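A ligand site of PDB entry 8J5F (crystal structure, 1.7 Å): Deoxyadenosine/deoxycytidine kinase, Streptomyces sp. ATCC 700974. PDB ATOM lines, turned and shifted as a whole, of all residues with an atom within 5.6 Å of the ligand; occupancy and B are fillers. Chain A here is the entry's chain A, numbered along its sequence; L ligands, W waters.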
ATOM      1  N   ASN A  36     -19.321  32.720 -21.735  1.00  0.00           N
ATOM      2  CA  ASN A  36     -19.988  31.466 -21.414  1.00  0.00           C
ATOM      3  C   ASN A  36     -19.031  30.479 -20.723  1.00  0.00           C
ATOM      4  O   ASN A  36     -17.800  30.628 -20.726  1.00  0.00           O
ATOM      5  CB  ASN A  36     -20.569  30.832 -22.681  1.00  0.00           C
ATOM      6  CG  ASN A  36     -21.786  29.947 -22.391  1.00  0.00           C
ATOM      7  OD1 ASN A  36     -22.330  29.960 -21.290  1.00  0.00           O
ATOM      8  ND2 ASN A  36     -22.191  29.172 -23.389  1.00  0.00           N
ATOM      9  N   THR A  37     -19.629  29.449 -20.137  1.00  0.00           N
ATOM     10  CA  THR A  37     -18.924  28.446 -19.355  1.00  0.00           C
ATOM     11  C   THR A  37     -17.818  27.759 -20.172  1.00  0.00           C
ATOM     12  O   THR A  37     -17.922  27.579 -21.389  1.00  0.00           O
ATOM     13  CB  THR A  37     -19.941  27.413 -18.851  1.00  0.00           C
ATOM     14  OG1 THR A  37     -19.302  26.398 -18.074  1.00  0.00           O
ATOM     15  CG2 THR A  37     -20.721  26.773 -20.027  1.00  0.00           C
ATOM     16  N   GLU A  64     -16.966  31.909  -9.291  1.00  0.00           N
ATOM     17  CA  GLU A  64     -18.312  31.722  -8.740  1.00  0.00           C
ATOM     18  C   GLU A  64     -18.396  30.490  -7.863  1.00  0.00           C
ATOM     19  O   GLU A  64     -19.226  30.443  -6.944  1.00  0.00           O
ATOM     20  CB  GLU A  64     -19.345  31.641  -9.866  1.00  0.00           C
ATOM     21  CG  GLU A  64     -19.501  32.927 -10.667  1.00  0.00           C
ATOM     22  CD  GLU A  64     -20.398  32.746 -11.886  1.00  0.00           C
ATOM     23  OE1 GLU A  64     -20.502  31.613 -12.401  1.00  0.00           O
ATOM     24  OE2 GLU A  64     -20.983  33.742 -12.342  1.00  0.00           O
ATOM     25  N   ARG A  65     -17.542  29.505  -8.094  1.00  0.00           N
ATOM     26  CA  ARG A  65     -17.578  28.278  -7.296  1.00  0.00           C
ATOM     27  C   ARG A  65     -17.349  28.564  -5.819  1.00  0.00           C
ATOM     28  O   ARG A  65     -17.777  27.771  -4.971  1.00  0.00           O
ATOM     29  CB  ARG A  65     -16.539  27.296  -7.863  1.00  0.00           C
ATOM     30  CG  ARG A  65     -16.693  25.855  -7.385  1.00  0.00           C
ATOM     31  CD  ARG A  65     -15.985  24.873  -8.325  1.00  0.00           C
ATOM     32  NE  ARG A  65     -16.657  24.738  -9.617  1.00  0.00           N
ATOM     33  CZ  ARG A  65     -17.730  23.999  -9.833  1.00  0.00           C
ATOM     34  NH1 ARG A  65     -18.301  23.294  -8.871  1.00  0.00           N
ATOM     35  NH2 ARG A  65     -18.276  23.969 -11.051  1.00  0.00           N
ATOM     36  N   HIS A  68     -21.109  29.168  -5.006  1.00  0.00           N
ATOM     37  CA  HIS A  68     -22.155  28.273  -5.497  1.00  0.00           C
ATOM     38  C   HIS A  68     -23.041  27.799  -4.350  1.00  0.00           C
ATOM     39  O   HIS A  68     -22.555  27.397  -3.300  1.00  0.00           O
ATOM     40  CB  HIS A  68     -21.571  27.019  -6.149  1.00  0.00           C
ATOM     41  CG  HIS A  68     -21.164  27.205  -7.576  1.00  0.00           C
ATOM     42  ND1 HIS A  68     -20.505  26.226  -8.287  1.00  0.00           N
ATOM     43  CD2 HIS A  68     -21.310  28.248  -8.419  1.00  0.00           C
ATOM     44  CE1 HIS A  68     -20.262  26.662  -9.509  1.00  0.00           C
ATOM     45  NE2 HIS A  68     -20.739  27.886  -9.607  1.00  0.00           N
ATOM     46  N   LEU A  72     -27.404  24.097  -6.057  1.00  0.00           N
ATOM     47  CA  LEU A  72     -27.204  24.452  -7.463  1.00  0.00           C
ATOM     48  C   LEU A  72     -27.853  23.464  -8.440  1.00  0.00           C
ATOM     49  O   LEU A  72     -28.536  23.869  -9.389  1.00  0.00           O
ATOM     50  CB  LEU A  72     -25.702  24.539  -7.748  1.00  0.00           C
ATOM     51  CG  LEU A  72     -25.317  24.862  -9.201  1.00  0.00           C
ATOM     52  CD1 LEU A  72     -25.855  26.235  -9.608  1.00  0.00           C
ATOM     53  CD2 LEU A  72     -23.816  24.806  -9.347  1.00  0.00           C
ATOM     54  N   MET A  75     -31.446  23.733  -9.727  1.00  0.00           N
ATOM     55  CA  MET A  75     -31.794  24.682 -10.777  1.00  0.00           C
ATOM     56  C   MET A  75     -31.868  24.008 -12.137  1.00  0.00           C
ATOM     57  O   MET A  75     -32.656  24.413 -13.000  1.00  0.00           O
ATOM     58  CB  MET A  75     -30.769  25.821 -10.830  1.00  0.00           C
ATOM     59  CG  MET A  75     -31.078  26.828 -11.935  1.00  0.00           C
ATOM     60  SD  MET A  75     -30.395  28.451 -11.683  1.00  0.00           S
ATOM     61  CE  MET A  75     -28.643  28.038 -11.785  1.00  0.00           C
ATOM     62  N   PHE A  76     -31.043  22.993 -12.365  1.00  0.00           N
ATOM     63  CA  PHE A  76     -31.009  22.350 -13.661  1.00  0.00           C
ATOM     64  C   PHE A  76     -31.851  21.082 -13.732  1.00  0.00           C
ATOM     65  O   PHE A  76     -32.219  20.673 -14.836  1.00  0.00           O
ATOM     66  CB  PHE A  76     -29.549  22.031 -14.054  1.00  0.00           C
ATOM     67  CG  PHE A  76     -28.683  23.258 -14.122  1.00  0.00           C
ATOM     68  CD1 PHE A  76     -29.061  24.364 -14.886  1.00  0.00           C
ATOM     69  CD2 PHE A  76     -27.506  23.324 -13.393  1.00  0.00           C
ATOM     70  CE1 PHE A  76     -28.258  25.519 -14.928  1.00  0.00           C
ATOM     71  CE2 PHE A  76     -26.702  24.465 -13.432  1.00  0.00           C
ATOM     72  CZ  PHE A  76     -27.083  25.562 -14.207  1.00  0.00           C
ATOM     73  N   GLN A  87     -31.093  31.753  -8.862  1.00  0.00           N
ATOM     74  CA  GLN A  87     -30.631  32.989  -9.499  1.00  0.00           C
ATOM     75  C   GLN A  87     -30.545  34.138  -8.501  1.00  0.00           C
ATOM     76  O   GLN A  87     -29.617  34.969  -8.557  1.00  0.00           O
ATOM     77  CB  GLN A  87     -31.528  33.375 -10.670  1.00  0.00           C
ATOM     78  CG  GLN A  87     -31.304  32.509 -11.910  1.00  0.00           C
ATOM     79  CD  GLN A  87     -29.875  32.572 -12.420  1.00  0.00           C
ATOM     80  OE1 GLN A  87     -29.233  33.634 -12.399  1.00  0.00           O
ATOM     81  NE2 GLN A  87     -29.366  31.442 -12.890  1.00  0.00           N
ATOM     82  N   PHE A  90     -27.141  33.585  -6.743  1.00  0.00           N
ATOM     83  CA  PHE A  90     -25.977  34.068  -7.487  1.00  0.00           C
ATOM     84  C   PHE A  90     -25.822  35.588  -7.361  1.00  0.00           C
ATOM     85  O   PHE A  90     -24.746  36.091  -7.005  1.00  0.00           O
ATOM     86  CB  PHE A  90     -26.086  33.689  -8.966  1.00  0.00           C
ATOM     87  CG  PHE A  90     -25.477  32.345  -9.333  1.00  0.00           C
ATOM     88  CD1 PHE A  90     -24.104  32.187  -9.433  1.00  0.00           C
ATOM     89  CD2 PHE A  90     -26.292  31.275  -9.658  1.00  0.00           C
ATOM     90  CE1 PHE A  90     -23.555  30.963  -9.787  1.00  0.00           C
ATOM     91  CE2 PHE A  90     -25.748  30.047 -10.035  1.00  0.00           C
ATOM     92  CZ  PHE A  90     -24.374  29.894 -10.103  1.00  0.00           C
ATOM     93  N   MET A  91     -26.905  36.329  -7.692  1.00  0.00           N
ATOM     94  CA  MET A  91     -26.934  37.779  -7.527  1.00  0.00           C
ATOM     95  C   MET A  91     -26.477  38.229  -6.148  1.00  0.00           C
ATOM     96  O   MET A  91     -25.626  39.129  -6.005  1.00  0.00           O
ATOM     97  CB  MET A  91     -28.358  38.287  -7.690  1.00  0.00           C
ATOM     98  CG  MET A  91     -28.464  39.801  -7.544  1.00  0.00           C
ATOM     99  SD  MET A  91     -30.015  40.443  -8.185  1.00  0.00           S
ATOM    100  CE  MET A  91     -31.148  39.669  -7.018  1.00  0.00           C
ATOM    101  N   ARG A  94     -22.794  37.278  -4.998  1.00  0.00           N
ATOM    102  CA  ARG A  94     -21.876  38.154  -5.733  1.00  0.00           C
ATOM    103  C   ARG A  94     -21.914  39.570  -5.184  1.00  0.00           C
ATOM    104  O   ARG A  94     -20.860  40.194  -4.962  1.00  0.00           O
ATOM    105  CB  ARG A  94     -22.229  38.160  -7.224  1.00  0.00           C
ATOM    106  CG  ARG A  94     -21.148  38.820  -8.080  1.00  0.00           C
ATOM    107  CD  ARG A  94     -21.648  39.129  -9.497  1.00  0.00           C
ATOM    108  NE  ARG A  94     -22.151  37.940 -10.166  1.00  0.00           N
ATOM    109  CZ  ARG A  94     -21.397  36.994 -10.708  1.00  0.00           C
ATOM    110  NH1 ARG A  94     -20.075  37.031 -10.636  1.00  0.00           N
ATOM    111  NH2 ARG A  94     -21.982  35.994 -11.370  1.00  0.00           N
ATOM    112  N   ARG A 113     -17.291  36.827 -14.310  1.00  0.00           N
ATOM    113  CA  ARG A 113     -18.471  37.599 -14.676  1.00  0.00           C
ATOM    114  C   ARG A 113     -18.505  38.910 -13.881  1.00  0.00           C
ATOM    115  O   ARG A 113     -17.780  39.056 -12.907  1.00  0.00           O
ATOM    116  CB  ARG A 113     -19.758  36.793 -14.448  1.00  0.00           C
ATOM    117  CG  ARG A 113     -20.092  35.906 -15.598  1.00  0.00           C
ATOM    118  CD  ARG A 113     -21.417  35.186 -15.398  1.00  0.00           C
ATOM    119  NE  ARG A 113     -21.189  33.799 -15.003  1.00  0.00           N
ATOM    120  CZ  ARG A 113     -20.803  32.854 -15.846  1.00  0.00           C
ATOM    121  NH1 ARG A 113     -20.607  33.107 -17.120  1.00  0.00           N
ATOM    122  NH2 ARG A 113     -20.606  31.619 -15.385  1.00  0.00           N
ATOM    123  N   ASP A 118     -25.555  38.707 -14.571  1.00  0.00           N
ATOM    124  CA  ASP A 118     -26.505  37.747 -13.993  1.00  0.00           C
ATOM    125  C   ASP A 118     -27.889  37.871 -14.616  1.00  0.00           C
ATOM    126  O   ASP A 118     -28.607  36.876 -14.734  1.00  0.00           O
ATOM    127  CB  ASP A 118     -26.601  37.918 -12.477  1.00  0.00           C
ATOM    128  CG  ASP A 118     -25.354  37.428 -11.746  1.00  0.00           C
ATOM    129  OD1 ASP A 118     -24.826  36.365 -12.117  1.00  0.00           O
ATOM    130  OD2 ASP A 118     -24.910  38.105 -10.796  1.00  0.00           O
ATOM    131  N   PHE A 121     -28.864  35.370 -17.274  1.00  0.00           N
ATOM    132  CA  PHE A 121     -29.223  34.022 -16.851  1.00  0.00           C
ATOM    133  C   PHE A 121     -30.673  33.940 -16.414  1.00  0.00           C
ATOM    134  O   PHE A 121     -31.322  32.921 -16.619  1.00  0.00           O
ATOM    135  CB  PHE A 121     -28.268  33.542 -15.754  1.00  0.00           C
ATOM    136  CG  PHE A 121     -26.866  33.257 -16.275  1.00  0.00           C
ATOM    137  CD1 PHE A 121     -25.935  34.284 -16.366  1.00  0.00           C
ATOM    138  CD2 PHE A 121     -26.504  31.988 -16.703  1.00  0.00           C
ATOM    139  CE1 PHE A 121     -24.664  34.048 -16.884  1.00  0.00           C
ATOM    140  CE2 PHE A 121     -25.236  31.739 -17.211  1.00  0.00           C
ATOM    141  CZ  PHE A 121     -24.311  32.772 -17.305  1.00  0.00           C
ATOM    142  N   HIS A 125     -34.043  31.608 -18.295  1.00  0.00           N
ATOM    143  CA  HIS A 125     -35.116  30.877 -17.623  1.00  0.00           C
ATOM    144  C   HIS A 125     -36.488  31.476 -17.918  1.00  0.00           C
ATOM    145  O   HIS A 125     -37.493  30.757 -17.931  1.00  0.00           O
ATOM    146  CB  HIS A 125     -34.871  30.838 -16.120  1.00  0.00           C
ATOM    147  CG  HIS A 125     -33.746  29.942 -15.696  1.00  0.00           C
ATOM    148  ND1 HIS A 125     -33.773  28.569 -15.895  1.00  0.00           N
ATOM    149  CD2 HIS A 125     -32.574  30.213 -15.072  1.00  0.00           C
ATOM    150  CE1 HIS A 125     -32.661  28.042 -15.404  1.00  0.00           C
ATOM    151  NE2 HIS A 125     -31.918  29.018 -14.911  1.00  0.00           N
ATOM    152  N   ARG A 179     -14.284  18.150 -12.494  1.00  0.00           N
ATOM    153  CA  ARG A 179     -15.421  19.002 -12.171  1.00  0.00           C
ATOM    154  C   ARG A 179     -16.654  18.135 -12.034  1.00  0.00           C
ATOM    155  O   ARG A 179     -16.761  17.100 -12.705  1.00  0.00           O
ATOM    156  CB  ARG A 179     -15.668  20.092 -13.228  1.00  0.00           C
ATOM    157  CG  ARG A 179     -16.407  19.626 -14.463  1.00  0.00           C
ATOM    158  CD  ARG A 179     -16.477  20.758 -15.459  1.00  0.00           C
ATOM    159  NE  ARG A 179     -17.529  21.719 -15.114  1.00  0.00           N
ATOM    160  CZ  ARG A 179     -17.306  23.013 -14.952  1.00  0.00           C
ATOM    161  NH1 ARG A 179     -16.086  23.521 -15.039  1.00  0.00           N
ATOM    162  NH2 ARG A 179     -18.326  23.827 -14.695  1.00  0.00           N
ATOM    163  N   GLU A 182     -23.158  18.674 -13.394  1.00  0.00           N
ATOM    164  CA  GLU A 182     -24.182  19.529 -12.826  1.00  0.00           C
ATOM    165  C   GLU A 182     -25.561  19.371 -13.466  1.00  0.00           C
ATOM    166  O   GLU A 182     -26.549  19.840 -12.899  1.00  0.00           O
ATOM    167  CB  GLU A 182     -23.753  20.997 -12.915  1.00  0.00           C
ATOM    168  CG  GLU A 182     -23.072  21.488 -11.642  1.00  0.00           C
ATOM    169  CD  GLU A 182     -22.010  22.549 -11.889  1.00  0.00           C
ATOM    170  OE1 GLU A 182     -22.119  23.290 -12.896  1.00  0.00           O
ATOM    171  OE2 GLU A 182     -21.092  22.661 -11.036  1.00  0.00           O
ATOM    172  N   PHE A 183     -25.661  18.727 -14.623  1.00  0.00           N
ATOM    173  CA  PHE A 183     -26.902  18.713 -15.364  1.00  0.00           C
ATOM    174  C   PHE A 183     -27.591  17.348 -15.290  1.00  0.00           C
ATOM    175  O   PHE A 183     -26.931  16.328 -15.063  1.00  0.00           O
ATOM    176  CB  PHE A 183     -26.622  19.107 -16.828  1.00  0.00           C
ATOM    177  CG  PHE A 183     -26.116  20.515 -16.975  1.00  0.00           C
ATOM    178  CD1 PHE A 183     -27.004  21.579 -17.055  1.00  0.00           C
ATOM    179  CD2 PHE A 183     -24.756  20.779 -17.026  1.00  0.00           C
ATOM    180  CE1 PHE A 183     -26.550  22.893 -17.180  1.00  0.00           C
ATOM    181  CE2 PHE A 183     -24.281  22.093 -17.163  1.00  0.00           C
ATOM    182  CZ  PHE A 183     -25.180  23.150 -17.235  1.00  0.00           C
ATOM    183  N   TRP A 196     -27.228  29.728 -23.570  1.00  0.00           N
ATOM    184  CA  TRP A 196     -26.382  30.751 -22.951  1.00  0.00           C
ATOM    185  C   TRP A 196     -25.445  31.405 -23.979  1.00  0.00           C
ATOM    186  O   TRP A 196     -25.201  32.613 -23.917  1.00  0.00           O
ATOM    187  CB  TRP A 196     -25.562  30.162 -21.811  1.00  0.00           C
ATOM    188  CG  TRP A 196     -26.320  29.789 -20.577  1.00  0.00           C
ATOM    189  CD1 TRP A 196     -27.478  30.356 -20.096  1.00  0.00           C
ATOM    190  CD2 TRP A 196     -25.959  28.765 -19.644  1.00  0.00           C
ATOM    191  NE1 TRP A 196     -27.850  29.733 -18.916  1.00  0.00           N
ATOM    192  CE2 TRP A 196     -26.938  28.747 -18.617  1.00  0.00           C
ATOM    193  CE3 TRP A 196     -24.900  27.854 -19.576  1.00  0.00           C
ATOM    194  CZ2 TRP A 196     -26.887  27.856 -17.539  1.00  0.00           C
ATOM    195  CZ3 TRP A 196     -24.845  26.961 -18.507  1.00  0.00           C
ATOM    196  CH2 TRP A 196     -25.829  26.976 -17.497  1.00  0.00           C
HETATM  197  O1  LIG L   1     -21.031  25.561 -12.891  1.00  0.00           O
HETATM  198  C1  LIG L   1     -21.781  26.731 -12.574  1.00  0.00           C
HETATM  199  C2  LIG L   1     -22.867  26.977 -13.600  1.00  0.00           C
HETATM  200  O2  LIG L   1     -23.706  28.078 -13.180  1.00  0.00           O
HETATM  201  C3  LIG L   1     -24.111  28.785 -14.333  1.00  0.00           C
HETATM  202  N1  LIG L   1     -24.578  30.110 -13.913  1.00  0.00           N
HETATM  203  C4  LIG L   1     -23.764  31.120 -13.603  1.00  0.00           C
HETATM  204  C5  LIG L   1     -24.148  32.478 -13.151  1.00  0.00           C
HETATM  205  C6  LIG L   1     -25.576  32.700 -13.028  1.00  0.00           C
HETATM  206  N2  LIG L   1     -26.389  31.519 -13.382  1.00  0.00           N
HETATM  207  C7  LIG L   1     -25.674  30.318 -13.787  1.00  0.00           C
HETATM  208  O3  LIG L   1     -26.578  29.321 -14.072  1.00  0.00           O
HETATM  209  N3  LIG L   1     -26.198  33.939 -12.598  1.00  0.00           N
HETATM  210  C8  LIG L   1     -22.881  28.751 -15.245  1.00  0.00           C
HETATM  211  O4  LIG L   1     -23.232  29.031 -16.583  1.00  0.00           O
HETATM  212  C9  LIG L   1     -22.368  27.320 -15.018  1.00  0.00           C
HETATM  213  O5  LIG L   1     -22.987  26.441 -15.951  1.00  0.00           O
HETATM  214  O   HOH W   1     -29.140  28.986 -15.003  1.00  0.00           O
HETATM  215  O   HOH W   2     -21.279  24.736 -17.016  1.00  0.00           O
HETATM  216  O   HOH W   3     -22.049  30.503 -18.585  1.00  0.00           O
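NE2 of Gln 87 sits at hydrogen-bond distance from N2 of the ligand, 3.0 Å away.
An oxygen (O1) of the ligand sits at hydrogen-bond distance from the side-chain carboxylate of Glu 182.
The side-chain carboxylate of Asp 118 sits at hydrogen-bond distance from a nitrogen (N3) of the ligand (2.8 Å).
The side-chain amide nitrogen (NE2) of Gln 87 sits at hydrogen-bond distance from the side-chain sulfur (SD) of Met 75, 3.4 Å away.
The side-chain carboxylate of Glu 64 is in salt-bridge range of the guanidinium group of Arg 94 (2.6 Å).
The guanidinium group (NE) of Arg 94 lies within salt-bridge range of the side-chain carboxylate (OD2) of Asp 118, at 2.8 Å.
The side-chain carboxylate (OE2) of Glu 64 lies within salt-bridge range of the guanidinium group (NE) of Arg 113 (2.7 Å).
OE2 of Glu 182 is in salt-bridge range of NH2 of Arg 65 (3.1 Å).
The side-chain sulfur (SD) of Met 75 is in hydrogen-bond range of a ring nitrogen (NE2) of His 125, at 3.6 Å.
OE2 of Glu 64 touches C5 of the ligand (3.5 Å).
Arg 65 touches the ligand.
His 68 touches the ligand.
Met 75 touches the ligand (CE to O3, 3.3 Å).
CZ of Phe 76 touches O3 of the ligand, at 3.8 Å.
Phe 90 touches the ligand.
Arg 113 touches the ligand (NH2 to C4, 3.7 Å).
Phe 121 touches the ligand.
Arg 179 touches the ligand (NH2 to O1, 3.7 Å).
Trp 196 touches the ligand.
Hydrophobic or aromatic side chains that line the ligand: His 68, Met 75, Phe 76, Phe 90, Phe 121 and Trp 196.
Within 4 Å of the ligand: Glu 64, Arg 65, His 68, Met 75, Phe 76, Gln 87, Phe 90, Arg 113, Asp 118, Phe 121, Arg 179, Glu 182 and Trp 196.
Along chain A the residues within 4 Å of the ligand span positions 64 to 196.
Water W2 lies within hydrogen-bond range of O5 of the ligand (2.6 Å) and OG1 of Thr 37 (2.8 Å).
Water W1 lies within hydrogen-bond range of O3 of the ligand, NE2 of His 125, NE2 of Gln 87 and SD of Met 75.
Water W3 lies within hydrogen-bond range of an oxygen (O4) of the ligand (2.8 Å), the side-chain amide oxygen of Asn 36 (2.8 Å), the backbone NH of Thr 37 (3.1 Å) and the guanidinium group of Arg 113 (3.3 Å).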
